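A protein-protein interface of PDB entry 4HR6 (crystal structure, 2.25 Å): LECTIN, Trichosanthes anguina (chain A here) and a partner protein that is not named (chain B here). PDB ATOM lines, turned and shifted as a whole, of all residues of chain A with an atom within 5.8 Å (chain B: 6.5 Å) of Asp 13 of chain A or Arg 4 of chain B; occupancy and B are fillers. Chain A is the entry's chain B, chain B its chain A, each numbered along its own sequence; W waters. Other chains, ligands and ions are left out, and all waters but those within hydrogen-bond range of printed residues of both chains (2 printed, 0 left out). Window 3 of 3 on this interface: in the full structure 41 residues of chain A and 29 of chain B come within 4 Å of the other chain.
O of Leu 3 of chain B touches CA of Leu 8 of chain A, at 3.5 Å.
Thr 9 of chain A touches Asn 2 of chain B (OG1 to OD1, 3.7 Å).
CA of Arg 4 of chain B touches O of Thr 9 of chain A (3.7 Å).
Leu 5 of chain B touches Asn 11 of chain A.
Water W1 lies within hydrogen-bond range of O of Ser 10 of chain A (2.8 Å), OG of Ser 6 of chain B (3.2 Å), N of Leu 5 of chain B (3.4 Å) and O of Thr 9 of chain A (3.4 Å).
Water W2 bridges the backbone carbonyl oxygen (O) of Leu 5 of chain B (2.9 Å) and the side-chain amide nitrogen (ND2) of Asn 11 of chain A (2.9 Å).
The guanidinium group (NH1) of Arg 4 of chain B lies within salt-bridge range of the side-chain carboxylate (OE2) of Glu 7 of chain B (3.9 Å).
The side-chain hydroxyl (OG) of Ser 15 of chain A sits at hydrogen-bond distance from the side-chain hydroxyl (OG1) of Thr 9 of chain A (2.5 Å).
Of the 9 printed residues of chain B, 5 touch a printed residue of chain A.
Among the printed residues, Asp or Glu carboxylates within 4 Å of a Lys or Arg side-chain nitrogen of the other chain: Asp 13 of chain A with Arg 4 of chain B (2.8 Å).
O of Thr 7 of chain A lies close to OD1 of Asn 2 of chain B (3.1 Å).
The backbone carbonyl oxygen (O) of Thr 7 of chain A sits at hydrogen-bond distance from the backbone NH (N) of Leu 3 of chain B (3.0 Å).
The backbone carbonyl oxygen (O) of Leu 3 of chain B is in hydrogen-bond range of the backbone NH (N) of Thr 9 of chain A.
The guanidinium group of Arg 4 of chain B lies within salt-bridge range of the side-chain carboxylate of Asp 13 of chain A (2.8 Å).
N of Leu 5 of chain B is in hydrogen-bond range of O of Thr 9 of chain A, at 3.0 Å.
The side-chain amide oxygen (OD1) of Asn 11 of chain A lies close to the side-chain hydroxyl (OG) of Ser 6 of chain B (3.4 Å).
Of the printed residues of chain A, Arg 4 of chain B touches Thr 9 (3.7 Å) and Asp 13 (2.8 Å).
Of the printed residues of chain A, Leu 5 of chain B touches Thr 9 and Asn 11.
Of the printed residues of chain A, Leu 3 of chain B touches Thr 7 (3.0 Å), Leu 8 (3.5 Å) and Thr 9 (2.9 Å).
Printed residues of chain B within 4 Å of Leu 8 of chain A: Leu 3 (3.5 Å).
Of the printed residues of chain B, Thr 7 of chain A touches Asn 2 and Leu 3.
Glu 14 of chain A touches none of the printed residues of chain B.
The nearest residue of chain A that does not touch Arg 4 of chain B is Thr 7 of chain A (5.6 Å).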
ATOM      1  N   THR A   7       4.605  16.979 -22.600  1.00  0.00           N
ATOM      2  CA  THR A   7       5.209  15.691 -22.925  1.00  0.00           C
ATOM      3  C   THR A   7       6.662  15.589 -22.461  1.00  0.00           C
ATOM      4  O   THR A   7       7.453  16.501 -22.627  1.00  0.00           O
ATOM      5  CB  THR A   7       5.109  15.432 -24.435  1.00  0.00           C
ATOM      6  OG1 THR A   7       3.728  15.486 -24.816  1.00  0.00           O
ATOM      7  CG2 THR A   7       5.655  14.059 -24.807  1.00  0.00           C
ATOM      8  N   LEU A   8       7.005  14.461 -21.864  1.00  0.00           N
ATOM      9  CA  LEU A   8       8.386  14.190 -21.479  1.00  0.00           C
ATOM     10  C   LEU A   8       8.789  12.901 -22.155  1.00  0.00           C
ATOM     11  O   LEU A   8       8.006  11.963 -22.193  1.00  0.00           O
ATOM     12  CB  LEU A   8       8.504  14.021 -19.973  1.00  0.00           C
ATOM     13  CG  LEU A   8       7.975  15.160 -19.117  1.00  0.00           C
ATOM     14  CD1 LEU A   8       7.790  14.659 -17.697  1.00  0.00           C
ATOM     15  CD2 LEU A   8       8.925  16.339 -19.153  1.00  0.00           C
ATOM     16  N   THR A   9      10.007  12.857 -22.683  1.00  0.00           N
ATOM     17  CA  THR A   9      10.516  11.686 -23.408  1.00  0.00           C
ATOM     18  C   THR A   9      11.868  11.238 -22.832  1.00  0.00           C
ATOM     19  O   THR A   9      12.805  12.018 -22.743  1.00  0.00           O
ATOM     20  CB  THR A   9      10.661  12.016 -24.894  1.00  0.00           C
ATOM     21  OG1 THR A   9       9.385  12.407 -25.404  1.00  0.00           O
ATOM     22  CG2 THR A   9      11.175  10.809 -25.697  1.00  0.00           C
ATOM     23  N   SER A  10      11.967   9.976 -22.445  1.00  0.00           N
ATOM     24  CA  SER A  10      13.205   9.452 -21.890  1.00  0.00           C
ATOM     25  C   SER A  10      14.260   9.223 -22.980  1.00  0.00           C
ATOM     26  O   SER A  10      13.985   9.374 -24.163  1.00  0.00           O
ATOM     27  CB  SER A  10      12.935   8.133 -21.171  1.00  0.00           C
ATOM     28  OG  SER A  10      12.733   7.112 -22.121  1.00  0.00           O
ATOM     29  N   ASN A  11      15.468   8.861 -22.546  1.00  0.00           N
ATOM     30  CA  ASN A  11      16.533   8.365 -23.437  1.00  0.00           C
ATOM     31  C   ASN A  11      16.236   7.031 -24.132  1.00  0.00           C
ATOM     32  O   ASN A  11      16.900   6.691 -25.093  1.00  0.00           O
ATOM     33  CB  ASN A  11      17.851   8.240 -22.675  1.00  0.00           C
ATOM     34  CG  ASN A  11      18.531   9.582 -22.486  1.00  0.00           C
ATOM     35  OD1 ASN A  11      19.025  10.175 -23.436  1.00  0.00           O
ATOM     36  ND2 ASN A  11      18.562  10.063 -21.261  1.00  0.00           N
ATOM     37  N   LYS A  12      15.250   6.277 -23.655  1.00  0.00           N
ATOM     38  CA  LYS A  12      14.764   5.104 -24.393  1.00  0.00           C
ATOM     39  C   LYS A  12      13.682   5.463 -25.422  1.00  0.00           C
ATOM     40  O   LYS A  12      13.057   4.570 -25.981  1.00  0.00           O
ATOM     41  CB  LYS A  12      14.212   4.055 -23.429  1.00  0.00           C
ATOM     42  CG  LYS A  12      15.250   3.470 -22.481  1.00  0.00           C
ATOM     43  CD  LYS A  12      14.618   2.815 -21.251  1.00  0.00           C
ATOM     44  CE  LYS A  12      13.776   1.599 -21.608  1.00  0.00           C
ATOM     45  NZ  LYS A  12      12.969   1.104 -20.449  1.00  0.00           N
ATOM     46  N   ASP A  13      13.463   6.757 -25.659  1.00  0.00           N
ATOM     47  CA  ASP A  13      12.346   7.252 -26.485  1.00  0.00           C
ATOM     48  C   ASP A  13      10.942   6.831 -26.028  1.00  0.00           C
ATOM     49  O   ASP A  13      10.061   6.656 -26.837  1.00  0.00           O
ATOM     50  CB  ASP A  13      12.548   6.872 -27.953  1.00  0.00           C
ATOM     51  CG  ASP A  13      13.623   7.680 -28.597  1.00  0.00           C
ATOM     52  OD1 ASP A  13      13.386   8.894 -28.792  1.00  0.00           O
ATOM     53  OD2 ASP A  13      14.699   7.103 -28.894  1.00  0.00           O
ATOM     54  N   GLU A  14      10.749   6.666 -24.729  1.00  0.00           N
ATOM     55  CA  GLU A  14       9.436   6.459 -24.170  1.00  0.00           C
ATOM     56  C   GLU A  14       8.868   7.841 -23.828  1.00  0.00           C
ATOM     57  O   GLU A  14       9.516   8.620 -23.117  1.00  0.00           O
ATOM     58  CB  GLU A  14       9.533   5.634 -22.902  1.00  0.00           C
ATOM     59  CG  GLU A  14      10.260   4.299 -23.021  1.00  0.00           C
ATOM     60  CD  GLU A  14      10.877   3.866 -21.696  1.00  0.00           C
ATOM     61  OE1 GLU A  14      11.510   4.726 -21.004  1.00  0.00           O
ATOM     62  OE2 GLU A  14      10.731   2.674 -21.344  1.00  0.00           O
ATOM     63  N   SER A  15       7.664   8.141 -24.308  1.00  0.00           N
ATOM     64  CA  SER A  15       7.003   9.422 -24.012  1.00  0.00           C
ATOM     65  C   SER A  15       5.806   9.248 -23.086  1.00  0.00           C
ATOM     66  O   SER A  15       5.020   8.314 -23.234  1.00  0.00           O
ATOM     67  CB  SER A  15       6.547  10.080 -25.296  1.00  0.00           C
ATOM     68  OG  SER A  15       7.643  10.664 -25.959  1.00  0.00           O
ATOM     69  N   ASN B   2       7.518  20.158 -24.690  1.00  0.00           N
ATOM     70  CA  ASN B   2       8.096  18.819 -24.744  1.00  0.00           C
ATOM     71  C   ASN B   2       9.532  18.883 -24.242  1.00  0.00           C
ATOM     72  O   ASN B   2      10.237  19.848 -24.511  1.00  0.00           O
ATOM     73  CB  ASN B   2       8.045  18.284 -26.186  1.00  0.00           C
ATOM     74  CG  ASN B   2       8.679  16.892 -26.340  1.00  0.00           C
ATOM     75  OD1 ASN B   2       8.547  16.011 -25.474  1.00  0.00           O
ATOM     76  ND2 ASN B   2       9.369  16.689 -27.459  1.00  0.00           N
ATOM     77  N   LEU B   3       9.950  17.876 -23.487  1.00  0.00           N
ATOM     78  CA  LEU B   3      11.314  17.797 -23.011  1.00  0.00           C
ATOM     79  C   LEU B   3      11.830  16.407 -23.354  1.00  0.00           C
ATOM     80  O   LEU B   3      11.354  15.411 -22.806  1.00  0.00           O
ATOM     81  CB  LEU B   3      11.356  18.070 -21.510  1.00  0.00           C
ATOM     82  CG  LEU B   3      12.633  18.553 -20.787  1.00  0.00           C
ATOM     83  CD1 LEU B   3      13.148  17.493 -19.842  1.00  0.00           C
ATOM     84  CD2 LEU B   3      13.742  19.072 -21.706  1.00  0.00           C
ATOM     85  N   ARG B   4      12.761  16.352 -24.303  1.00  0.00           N
ATOM     86  CA  ARG B   4      13.409  15.106 -24.713  1.00  0.00           C
ATOM     87  C   ARG B   4      14.765  15.025 -24.026  1.00  0.00           C
ATOM     88  O   ARG B   4      15.612  15.897 -24.210  1.00  0.00           O
ATOM     89  CB  ARG B   4      13.607  15.058 -26.225  1.00  0.00           C
ATOM     90  CG  ARG B   4      12.356  15.291 -27.065  1.00  0.00           C
ATOM     91  CD  ARG B   4      12.619  15.118 -28.563  1.00  0.00           C
ATOM     92  NE  ARG B   4      12.645  13.700 -28.946  1.00  0.00           N
ATOM     93  CZ  ARG B   4      13.738  12.929 -29.023  1.00  0.00           C
ATOM     94  NH1 ARG B   4      14.953  13.415 -28.773  1.00  0.00           N
ATOM     95  NH2 ARG B   4      13.613  11.649 -29.361  1.00  0.00           N
ATOM     96  N   LEU B   5      14.983  13.988 -23.233  1.00  0.00           N
ATOM     97  CA  LEU B   5      16.233  13.904 -22.500  1.00  0.00           C
ATOM     98  C   LEU B   5      17.462  13.608 -23.376  1.00  0.00           C
ATOM     99  O   LEU B   5      18.558  14.009 -23.009  1.00  0.00           O
ATOM    100  CB  LEU B   5      16.129  12.923 -21.341  1.00  0.00           C
ATOM    101  CG  LEU B   5      15.254  13.432 -20.195  1.00  0.00           C
ATOM    102  CD1 LEU B   5      15.246  12.416 -19.065  1.00  0.00           C
ATOM    103  CD2 LEU B   5      15.757  14.785 -19.701  1.00  0.00           C
ATOM    104  N   SER B   6      17.286  12.947 -24.523  1.00  0.00           N
ATOM    105  CA  SER B   6      18.413  12.684 -25.455  1.00  0.00           C
ATOM    106  C   SER B   6      19.176  13.947 -25.840  1.00  0.00           C
ATOM    107  O   SER B   6      20.396  14.009 -25.728  1.00  0.00           O
ATOM    108  CB  SER B   6      17.921  12.002 -26.735  1.00  0.00           C
ATOM    109  OG  SER B   6      17.538  10.670 -26.451  1.00  0.00           O
ATOM    110  N   GLU B   7      18.440  14.956 -26.276  1.00  0.00           N
ATOM    111  CA  GLU B   7      19.043  16.193 -26.752  1.00  0.00           C
ATOM    112  C   GLU B   7      18.989  17.276 -25.665  1.00  0.00           C
ATOM    113  O   GLU B   7      18.703  18.434 -25.945  1.00  0.00           O
ATOM    114  CB  GLU B   7      18.370  16.647 -28.069  1.00  0.00           C
ATOM    115  CG  GLU B   7      16.847  16.779 -28.031  1.00  0.00           C
ATOM    116  CD  GLU B   7      16.232  17.133 -29.384  1.00  0.00           C
ATOM    117  OE1 GLU B   7      16.978  17.313 -30.379  1.00  0.00           O
ATOM    118  OE2 GLU B   7      14.987  17.239 -29.454  1.00  0.00           O
ATOM    119  N   ALA B   8      19.307  16.894 -24.430  1.00  0.00           N
ATOM    120  CA  ALA B   8      19.074  17.752 -23.267  1.00  0.00           C
ATOM    121  C   ALA B   8      20.339  18.216 -22.561  1.00  0.00           C
ATOM    122  O   ALA B   8      21.166  17.412 -22.136  1.00  0.00           O
ATOM    123  CB  ALA B   8      18.189  17.037 -22.268  1.00  0.00           C
ATOM    124  N   ASN B   9      20.465  19.526 -22.428  1.00  0.00           N
ATOM    125  CA  ASN B   9      21.479  20.126 -21.573  1.00  0.00           C
ATOM    126  C   ASN B   9      20.840  21.267 -20.782  1.00  0.00           C
ATOM    127  O   ASN B   9      19.653  21.545 -20.947  1.00  0.00           O
ATOM    128  CB  ASN B   9      22.654  20.633 -22.417  1.00  0.00           C
ATOM    129  CG  ASN B   9      22.210  21.526 -23.555  1.00  0.00           C
ATOM    130  OD1 ASN B   9      21.649  22.604 -23.345  1.00  0.00           O
ATOM    131  ND2 ASN B   9      22.452  21.079 -24.774  1.00  0.00           N
ATOM    132  N   THR B  12      18.682  23.688 -22.936  1.00  0.00           N
ATOM    133  CA  THR B  12      17.373  23.239 -23.430  1.00  0.00           C
ATOM    134  C   THR B  12      16.394  23.035 -22.262  1.00  0.00           C
ATOM    135  O   THR B  12      15.220  23.263 -22.417  1.00  0.00           O
ATOM    136  CB  THR B  12      17.464  21.941 -24.263  1.00  0.00           C
ATOM    137  OG1 THR B  12      17.922  20.878 -23.425  1.00  0.00           O
ATOM    138  CG2 THR B  12      18.442  22.116 -25.438  1.00  0.00           C
HETATM  139  O   HOH W   1      14.542  11.642 -25.686  1.00  0.00           O
HETATM  140  O   HOH W   2      20.056  12.585 -21.017  1.00  0.00           O
